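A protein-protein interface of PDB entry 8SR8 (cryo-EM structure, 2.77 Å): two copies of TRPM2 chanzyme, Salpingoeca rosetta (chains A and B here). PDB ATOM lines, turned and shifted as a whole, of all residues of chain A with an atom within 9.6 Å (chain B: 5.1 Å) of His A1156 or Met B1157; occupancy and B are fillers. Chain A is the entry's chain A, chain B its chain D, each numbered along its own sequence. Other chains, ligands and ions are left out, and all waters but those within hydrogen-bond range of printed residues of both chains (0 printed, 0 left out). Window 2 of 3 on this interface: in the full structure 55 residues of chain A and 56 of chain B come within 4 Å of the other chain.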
ATOM      1  N   GLN A 389      20.801 -20.693 -21.523  1.00  0.00           N
ATOM      2  CA  GLN A 389      19.838 -19.623 -21.780  1.00  0.00           C
ATOM      3  C   GLN A 389      19.162 -19.063 -20.529  1.00  0.00           C
ATOM      4  O   GLN A 389      18.453 -18.058 -20.638  1.00  0.00           O
ATOM      5  CB  GLN A 389      18.749 -20.116 -22.745  1.00  0.00           C
ATOM      6  CG  GLN A 389      17.770 -21.162 -22.180  1.00  0.00           C
ATOM      7  CD  GLN A 389      18.234 -22.616 -22.279  1.00  0.00           C
ATOM      8  OE1 GLN A 389      19.410 -22.910 -22.499  1.00  0.00           O
ATOM      9  NE2 GLN A 389      17.292 -23.535 -22.116  1.00  0.00           N
ATOM     10  N   GLU A 390      19.356 -19.667 -19.359  1.00  0.00           N
ATOM     11  CA  GLU A 390      18.764 -19.197 -18.116  1.00  0.00           C
ATOM     12  C   GLU A 390      19.806 -18.681 -17.138  1.00  0.00           C
ATOM     13  O   GLU A 390      19.683 -17.560 -16.633  1.00  0.00           O
ATOM     14  CB  GLU A 390      17.949 -20.323 -17.463  1.00  0.00           C
ATOM     15  N   GLY A1148      29.502  -7.121 -24.196  1.00  0.00           N
ATOM     16  CA  GLY A1148      28.764  -8.182 -23.496  1.00  0.00           C
ATOM     17  C   GLY A1148      27.255  -7.999 -23.583  1.00  0.00           C
ATOM     18  O   GLY A1148      26.503  -8.974 -23.775  1.00  0.00           O
ATOM     19  N   MET A1149      26.803  -6.744 -23.400  1.00  0.00           N
ATOM     20  CA  MET A1149      25.391  -6.383 -23.500  1.00  0.00           C
ATOM     21  C   MET A1149      24.878  -6.543 -24.940  1.00  0.00           C
ATOM     22  O   MET A1149      23.720  -6.949 -25.139  1.00  0.00           O
ATOM     23  CB  MET A1149      25.206  -4.968 -22.966  1.00  0.00           C
ATOM     24  CG  MET A1149      23.843  -4.704 -22.396  1.00  0.00           C
ATOM     25  SD  MET A1149      23.705  -3.055 -21.698  1.00  0.00           S
ATOM     26  CE  MET A1149      24.912  -3.147 -20.384  1.00  0.00           C
ATOM     27  N   MET A1150      25.734  -6.228 -25.939  1.00  0.00           N
ATOM     28  CA  MET A1150      25.420  -6.483 -27.355  1.00  0.00           C
ATOM     29  C   MET A1150      25.303  -7.973 -27.676  1.00  0.00           C
ATOM     30  O   MET A1150      24.567  -8.339 -28.602  1.00  0.00           O
ATOM     31  CB  MET A1150      26.441  -5.880 -28.300  1.00  0.00           C
ATOM     32  CG  MET A1150      26.509  -4.415 -28.390  1.00  0.00           C
ATOM     33  SD  MET A1150      27.808  -4.134 -29.583  1.00  0.00           S
ATOM     34  CE  MET A1150      27.865  -2.375 -29.542  1.00  0.00           C
ATOM     35  N   ASP A1151      26.155  -8.803 -27.040  1.00  0.00           N
ATOM     36  CA  ASP A1151      26.097 -10.265 -27.178  1.00  0.00           C
ATOM     37  C   ASP A1151      24.762 -10.822 -26.683  1.00  0.00           C
ATOM     38  O   ASP A1151      24.188 -11.717 -27.329  1.00  0.00           O
ATOM     39  CB  ASP A1151      27.263 -10.918 -26.438  1.00  0.00           C
ATOM     40  N   GLN A1152      24.291 -10.309 -25.520  1.00  0.00           N
ATOM     41  CA  GLN A1152      22.965 -10.636 -24.961  1.00  0.00           C
ATOM     42  C   GLN A1152      21.839 -10.208 -25.908  1.00  0.00           C
ATOM     43  O   GLN A1152      20.827 -10.924 -26.053  1.00  0.00           O
ATOM     44  CB  GLN A1152      22.774  -9.995 -23.588  1.00  0.00           C
ATOM     45  CG  GLN A1152      23.694 -10.539 -22.517  1.00  0.00           C
ATOM     46  CD  GLN A1152      23.995  -9.515 -21.447  1.00  0.00           C
ATOM     47  OE1 GLN A1152      23.466  -8.406 -21.468  1.00  0.00           O
ATOM     48  NE2 GLN A1152      24.851  -9.883 -20.500  1.00  0.00           N
ATOM     49  N   LEU A1153      22.002  -9.003 -26.496  1.00  0.00           N
ATOM     50  CA  LEU A1153      21.084  -8.418 -27.478  1.00  0.00           C
ATOM     51  C   LEU A1153      20.980  -9.295 -28.731  1.00  0.00           C
ATOM     52  O   LEU A1153      19.886  -9.466 -29.285  1.00  0.00           O
ATOM     53  CB  LEU A1153      21.565  -7.015 -27.838  1.00  0.00           C
ATOM     54  CG  LEU A1153      20.615  -5.947 -28.348  1.00  0.00           C
ATOM     55  CD1 LEU A1153      19.472  -5.833 -27.394  1.00  0.00           C
ATOM     56  CD2 LEU A1153      21.350  -4.641 -28.428  1.00  0.00           C
ATOM     57  N   LEU A1154      22.133  -9.811 -29.202  1.00  0.00           N
ATOM     58  CA  LEU A1154      22.203 -10.684 -30.378  1.00  0.00           C
ATOM     59  C   LEU A1154      21.535 -12.032 -30.120  1.00  0.00           C
ATOM     60  O   LEU A1154      20.994 -12.632 -31.061  1.00  0.00           O
ATOM     61  CB  LEU A1154      23.648 -10.905 -30.806  1.00  0.00           C
ATOM     62  CG  LEU A1154      24.307  -9.890 -31.723  1.00  0.00           C
ATOM     63  CD1 LEU A1154      25.751 -10.267 -31.868  1.00  0.00           C
ATOM     64  CD2 LEU A1154      23.630  -9.961 -33.064  1.00  0.00           C
ATOM     65  N   GLU A1155      21.675 -12.560 -28.880  1.00  0.00           N
ATOM     66  CA  GLU A1155      20.970 -13.782 -28.455  1.00  0.00           C
ATOM     67  C   GLU A1155      19.453 -13.601 -28.496  1.00  0.00           C
ATOM     68  O   GLU A1155      18.721 -14.533 -28.880  1.00  0.00           O
ATOM     69  CB  GLU A1155      21.413 -14.236 -27.062  1.00  0.00           C
ATOM     70  CG  GLU A1155      22.839 -14.775 -26.974  1.00  0.00           C
ATOM     71  CD  GLU A1155      23.054 -16.088 -27.716  1.00  0.00           C
ATOM     72  OE1 GLU A1155      22.117 -16.913 -27.789  1.00  0.00           O
ATOM     73  OE2 GLU A1155      24.172 -16.296 -28.233  1.00  0.00           O
ATOM     74  N   HIS A1156      18.970 -12.445 -28.000  1.00  0.00           N
ATOM     75  CA  HIS A1156      17.539 -12.126 -28.063  1.00  0.00           C
ATOM     76  C   HIS A1156      17.054 -11.956 -29.508  1.00  0.00           C
ATOM     77  O   HIS A1156      15.946 -12.397 -29.849  1.00  0.00           O
ATOM     78  CB  HIS A1156      17.253 -10.852 -27.275  1.00  0.00           C
ATOM     79  CG  HIS A1156      17.095 -11.069 -25.806  1.00  0.00           C
ATOM     80  ND1 HIS A1156      16.202 -10.350 -25.042  1.00  0.00           N
ATOM     81  CD2 HIS A1156      17.712 -11.924 -24.959  1.00  0.00           C
ATOM     82  CE1 HIS A1156      16.277 -10.752 -23.787  1.00  0.00           C
ATOM     83  NE2 HIS A1156      17.187 -11.707 -23.709  1.00  0.00           N
ATOM     84  N   MET A1157      17.900 -11.338 -30.353  1.00  0.00           N
ATOM     85  CA  MET A1157      17.664 -11.159 -31.791  1.00  0.00           C
ATOM     86  C   MET A1157      17.537 -12.477 -32.565  1.00  0.00           C
ATOM     87  O   MET A1157      16.656 -12.604 -33.431  1.00  0.00           O
ATOM     88  CB  MET A1157      18.781 -10.291 -32.357  1.00  0.00           C
ATOM     89  CG  MET A1157      18.362  -9.501 -33.552  1.00  0.00           C
ATOM     90  SD  MET A1157      17.085  -8.401 -32.907  1.00  0.00           S
ATOM     91  CE  MET A1157      18.027  -7.363 -31.810  1.00  0.00           C
ATOM     92  N   ILE A1158      18.480 -13.421 -32.332  1.00  0.00           N
ATOM     93  CA  ILE A1158      18.476 -14.746 -32.980  1.00  0.00           C
ATOM     94  C   ILE A1158      17.244 -15.555 -32.512  1.00  0.00           C
ATOM     95  O   ILE A1158      16.701 -16.370 -33.284  1.00  0.00           O
ATOM     96  CB  ILE A1158      19.858 -15.458 -32.874  1.00  0.00           C
ATOM     97  CG1 ILE A1158      19.981 -16.633 -33.864  1.00  0.00           C
ATOM     98  CG2 ILE A1158      20.215 -15.987 -31.509  1.00  0.00           C
ATOM     99  CD1 ILE A1158      21.378 -17.248 -34.001  1.00  0.00           C
ATOM    100  N   SER A1159      16.835 -15.372 -31.218  1.00  0.00           N
ATOM    101  CA  SER A1159      15.604 -15.963 -30.660  1.00  0.00           C
ATOM    102  C   SER A1159      14.363 -15.457 -31.414  1.00  0.00           C
ATOM    103  O   SER A1159      13.436 -16.241 -31.669  1.00  0.00           O
ATOM    104  CB  SER A1159      15.494 -15.675 -29.166  1.00  0.00           C
ATOM    105  OG  SER A1159      16.395 -16.484 -28.434  1.00  0.00           O
ATOM    106  N   PHE A1160      14.324 -14.171 -31.753  1.00  0.00           N
ATOM    107  CA  PHE A1160      13.162 -13.702 -32.545  1.00  0.00           C
ATOM    108  C   PHE A1160      13.259 -14.293 -33.950  1.00  0.00           C
ATOM    109  O   PHE A1160      12.243 -14.725 -34.489  1.00  0.00           O
ATOM    110  CB  PHE A1160      13.085 -12.180 -32.614  1.00  0.00           C
ATOM    111  CG  PHE A1160      12.632 -11.518 -31.342  1.00  0.00           C
ATOM    112  CD1 PHE A1160      11.545 -12.008 -30.639  1.00  0.00           C
ATOM    113  CD2 PHE A1160      13.294 -10.408 -30.847  1.00  0.00           C
ATOM    114  CE1 PHE A1160      11.131 -11.400 -29.466  1.00  0.00           C
ATOM    115  CE2 PHE A1160      12.879  -9.801 -29.673  1.00  0.00           C
ATOM    116  CZ  PHE A1160      11.800 -10.299 -28.987  1.00  0.00           C
ATOM    117  N   ARG A1161      14.460 -14.291 -34.520  1.00  0.00           N
ATOM    118  CA  ARG A1161      14.625 -14.846 -35.872  1.00  0.00           C
ATOM    119  C   ARG A1161      14.038 -16.252 -35.960  1.00  0.00           C
ATOM    120  O   ARG A1161      13.354 -16.577 -36.945  1.00  0.00           O
ATOM    121  CB  ARG A1161      16.101 -14.851 -36.268  1.00  0.00           C
ATOM    122  N   PHE A1162      14.323 -17.081 -34.935  1.00  0.00           N
ATOM    123  CA  PHE A1162      13.765 -18.430 -34.811  1.00  0.00           C
ATOM    124  C   PHE A1162      12.246 -18.399 -34.637  1.00  0.00           C
ATOM    125  O   PHE A1162      11.538 -19.232 -35.221  1.00  0.00           O
ATOM    126  CB  PHE A1162      14.401 -19.160 -33.635  1.00  0.00           C
ATOM    127  CG  PHE A1162      13.975 -20.584 -33.524  1.00  0.00           C
ATOM    128  CD1 PHE A1162      14.316 -21.503 -34.526  1.00  0.00           C
ATOM    129  CD2 PHE A1162      13.202 -20.999 -32.429  1.00  0.00           C
ATOM    130  CE1 PHE A1162      13.907 -22.841 -34.435  1.00  0.00           C
ATOM    131  CE2 PHE A1162      12.783 -22.332 -32.316  1.00  0.00           C
ATOM    132  CZ  PHE A1162      13.139 -23.252 -33.324  1.00  0.00           C
ATOM    133  N   SER A1163      11.757 -17.480 -33.776  1.00  0.00           N
ATOM    134  CA  SER A1163      10.328 -17.311 -33.492  1.00  0.00           C
ATOM    135  C   SER A1163       9.545 -16.843 -34.719  1.00  0.00           C
ATOM    136  O   SER A1163       8.415 -17.295 -34.947  1.00  0.00           O
ATOM    137  CB  SER A1163      10.134 -16.331 -32.338  1.00  0.00           C
ATOM    138  OG  SER A1163      10.686 -16.844 -31.141  1.00  0.00           O
ATOM    139  N   LEU A1164      10.107 -15.882 -35.471  1.00  0.00           N
ATOM    140  CA  LEU A1164       9.490 -15.388 -36.699  1.00  0.00           C
ATOM    141  C   LEU A1164       9.508 -16.442 -37.801  1.00  0.00           C
ATOM    142  O   LEU A1164       8.610 -16.449 -38.654  1.00  0.00           O
ATOM    143  CB  LEU A1164      10.195 -14.116 -37.164  1.00  0.00           C
ATOM    144  N   LEU B1153      17.098  -0.012 -24.970  1.00  0.00           N
ATOM    145  CA  LEU B1153      16.974  -0.953 -26.088  1.00  0.00           C
ATOM    146  C   LEU B1153      16.572  -2.348 -25.595  1.00  0.00           C
ATOM    147  O   LEU B1153      15.751  -3.023 -26.230  1.00  0.00           O
ATOM    148  CB  LEU B1153      18.298  -1.008 -26.844  1.00  0.00           C
ATOM    149  CG  LEU B1153      18.370  -1.404 -28.308  1.00  0.00           C
ATOM    150  CD1 LEU B1153      17.412  -0.555 -29.077  1.00  0.00           C
ATOM    151  CD2 LEU B1153      19.768  -1.178 -28.804  1.00  0.00           C
ATOM    152  N   LEU B1154      17.189  -2.795 -24.483  1.00  0.00           N
ATOM    153  CA  LEU B1154      16.905  -4.097 -23.872  1.00  0.00           C
ATOM    154  C   LEU B1154      15.496  -4.149 -23.287  1.00  0.00           C
ATOM    155  O   LEU B1154      14.886  -5.229 -23.266  1.00  0.00           O
ATOM    156  CB  LEU B1154      17.921  -4.422 -22.785  1.00  0.00           C
ATOM    157  CG  LEU B1154      19.233  -5.075 -23.176  1.00  0.00           C
ATOM    158  CD1 LEU B1154      20.096  -5.152 -21.952  1.00  0.00           C
ATOM    159  CD2 LEU B1154      18.936  -6.465 -23.671  1.00  0.00           C
ATOM    160  N   GLU B1155      15.029  -3.017 -22.707  1.00  0.00           N
ATOM    161  CA  GLU B1155      13.641  -2.887 -22.227  1.00  0.00           C
ATOM    162  C   GLU B1155      12.634  -3.035 -23.368  1.00  0.00           C
ATOM    163  O   GLU B1155      11.565  -3.647 -23.184  1.00  0.00           O
ATOM    164  CB  GLU B1155      13.419  -1.563 -21.492  1.00  0.00           C
ATOM    165  CG  GLU B1155      14.120  -1.442 -20.141  1.00  0.00           C
ATOM    166  CD  GLU B1155      13.580  -2.384 -19.073  1.00  0.00           C
ATOM    167  OE1 GLU B1155      12.368  -2.692 -19.081  1.00  0.00           O
ATOM    168  OE2 GLU B1155      14.377  -2.825 -18.219  1.00  0.00           O
ATOM    169  N   HIS B1156      12.921  -2.386 -24.514  1.00  0.00           N
ATOM    170  CA  HIS B1156      12.070  -2.523 -25.701  1.00  0.00           C
ATOM    171  C   HIS B1156      12.090  -3.952 -26.257  1.00  0.00           C
ATOM    172  O   HIS B1156      11.047  -4.469 -26.684  1.00  0.00           O
ATOM    173  CB  HIS B1156      12.524  -1.548 -26.784  1.00  0.00           C
ATOM    174  CG  HIS B1156      11.990  -0.164 -26.616  1.00  0.00           C
ATOM    175  ND1 HIS B1156      11.641   0.631 -27.686  1.00  0.00           N
ATOM    176  CD2 HIS B1156      11.744   0.569 -25.506  1.00  0.00           C
ATOM    177  CE1 HIS B1156      11.204   1.795 -27.241  1.00  0.00           C
ATOM    178  NE2 HIS B1156      11.256   1.783 -25.921  1.00  0.00           N
ATOM    179  N   MET B1157      13.275  -4.589 -26.222  1.00  0.00           N
ATOM    180  CA  MET B1157      13.485  -5.988 -26.620  1.00  0.00           C
ATOM    181  C   MET B1157      12.692  -6.995 -25.777  1.00  0.00           C
ATOM    182  O   MET B1157      12.118  -7.949 -26.328  1.00  0.00           O
ATOM    183  CB  MET B1157      14.978  -6.282 -26.574  1.00  0.00           C
ATOM    184  CG  MET B1157      15.397  -7.349 -27.530  1.00  0.00           C
ATOM    185  SD  MET B1157      15.028  -6.638 -29.147  1.00  0.00           S
ATOM    186  CE  MET B1157      16.187  -5.290 -29.218  1.00  0.00           C
ATOM    187  N   ILE B1158      12.747  -6.849 -24.432  1.00  0.00           N
ATOM    188  CA  ILE B1158      12.019  -7.724 -23.492  1.00  0.00           C
ATOM    189  C   ILE B1158      10.496  -7.525 -23.666  1.00  0.00           C
ATOM    190  O   ILE B1158       9.714  -8.478 -23.474  1.00  0.00           O
ATOM    191  CB  ILE B1158      12.574  -7.618 -22.040  1.00  0.00           C
ATOM    192  CG1 ILE B1158      12.099  -8.789 -21.154  1.00  0.00           C
ATOM    193  CG2 ILE B1158      12.243  -6.344 -21.307  1.00  0.00           C
ATOM    194  CD1 ILE B1158      12.773  -8.903 -19.783  1.00  0.00           C
ATOM    195  N   SER B1159      10.064  -6.263 -23.976  1.00  0.00           N
ATOM    196  CA  SER B1159       8.663  -5.937 -24.306  1.00  0.00           C
ATOM    197  C   SER B1159       8.205  -6.699 -25.560  1.00  0.00           C
ATOM    198  O   SER B1159       7.060  -7.176 -25.606  1.00  0.00           O
ATOM    199  CB  SER B1159       8.483  -4.433 -24.482  1.00  0.00           C
ATOM    200  OG  SER B1159       8.500  -3.778 -23.228  1.00  0.00           O
ATOM    201  N   PHE B1160       9.062  -6.803 -26.572  1.00  0.00           N
ATOM    202  CA  PHE B1160       8.645  -7.603 -27.749  1.00  0.00           C
ATOM    203  C   PHE B1160       8.604  -9.076 -27.349  1.00  0.00           C
ATOM    204  O   PHE B1160       7.672  -9.776 -27.737  1.00  0.00           O
ATOM    205  CB  PHE B1160       9.575  -7.404 -28.943  1.00  0.00           C
ATOM    206  CG  PHE B1160       9.420  -6.080 -29.641  1.00  0.00           C
ATOM    207  CD1 PHE B1160       8.165  -5.582 -29.940  1.00  0.00           C
ATOM    208  CD2 PHE B1160      10.531  -5.335 -29.996  1.00  0.00           C
ATOM    209  CE1 PHE B1160       8.025  -4.362 -30.581  1.00  0.00           C
ATOM    210  CE2 PHE B1160      10.389  -4.114 -30.636  1.00  0.00           C
ATOM    211  CZ  PHE B1160       9.137  -3.632 -30.925  1.00  0.00           C
ATOM    212  N   ARG B1161       9.608  -9.523 -26.600  1.00  0.00           N
ATOM    213  CA  ARG B1161       9.630 -10.931 -26.177  1.00  0.00           C
ATOM    214  C   ARG B1161       8.310 -11.325 -25.521  1.00  0.00           C
ATOM    215  O   ARG B1161       7.777 -12.411 -25.803  1.00  0.00           O
ATOM    216  CB  ARG B1161      10.800 -11.183 -25.228  1.00  0.00           C
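Among the printed residues, merely in contact across the chains: Phe A1160 with Arg B1161, Phe A1160 with Met B1157, Phe A1160 with Phe B1160, Met A1157 with Met B1157, Leu A1153 with Met B1157, Met A1149 with Leu B1154, Leu A1153 with Leu B1154, Leu A1153 with Leu B1153 and His A1156 with Met B1157.
Leu A1153 touches Leu B1154, but with the chains exchanged Leu A1154 does not touch Leu B1153 (9.0 Å).
His A1156 touches Met B1157, but with the chains exchanged Met A1157 does not touch His B1156 (8.8 Å).
Met B1157 touches its own counterpart, Met A1157.
Phe A1160 touches Arg B1161, but with the chains exchanged Arg A1161 does not touch Phe B1160 (10.1 Å).
Positions printed for both chains: 1153, 1154, 1155, 1156, 1157, 1158, 1159, 1160 and 1161.
Hydrophobic or aromatic side chains of chain A within 4 Å of the printed part of chain B: Met A1149, Leu A1153, His A1156, Met A1157 and Phe A1160.
Of the 9 printed residues of chain B, 5 touch a printed residue of chain A.
Printed residues of chain B that touch a printed residue of chain A: Leu B1153, Leu B1154, Met B1157, Phe B1160 and Arg B1161.
Hydrophobic or aromatic side chains of chain B within 4 Å of the printed part of chain A: Leu B1153, Leu B1154, Met B1157 and Phe B1160.
Among the printed residues, 9 pairs touch across the chains.
His A1156 touches just one residue of chain B: Met B1157 (3.97 Å).
Arg A1161 touches none of the printed residues of chain B.
Phe A1162 touches none of the printed residues of chain B.
Of the printed residues of chain A, Leu B1154 touches Met A1149 and Leu A1153.
Printed residues of chain A within 4 Å of Met B1157: Leu A1153 (3.8 Å), His A1156 (3.97 Å), Met A1157 (3.8 Å) and Phe A1160 (3.6 Å).
Printed residues of chain A within 4 Å of Phe B1160: Phe A1160 (3.7 Å).
Of the printed residues of chain A, Arg B1161 touches Phe A1160 (3.3 Å).
The nearest printed residue of chain A that does not touch Arg B1161 is His A1156 (5.5 Å).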
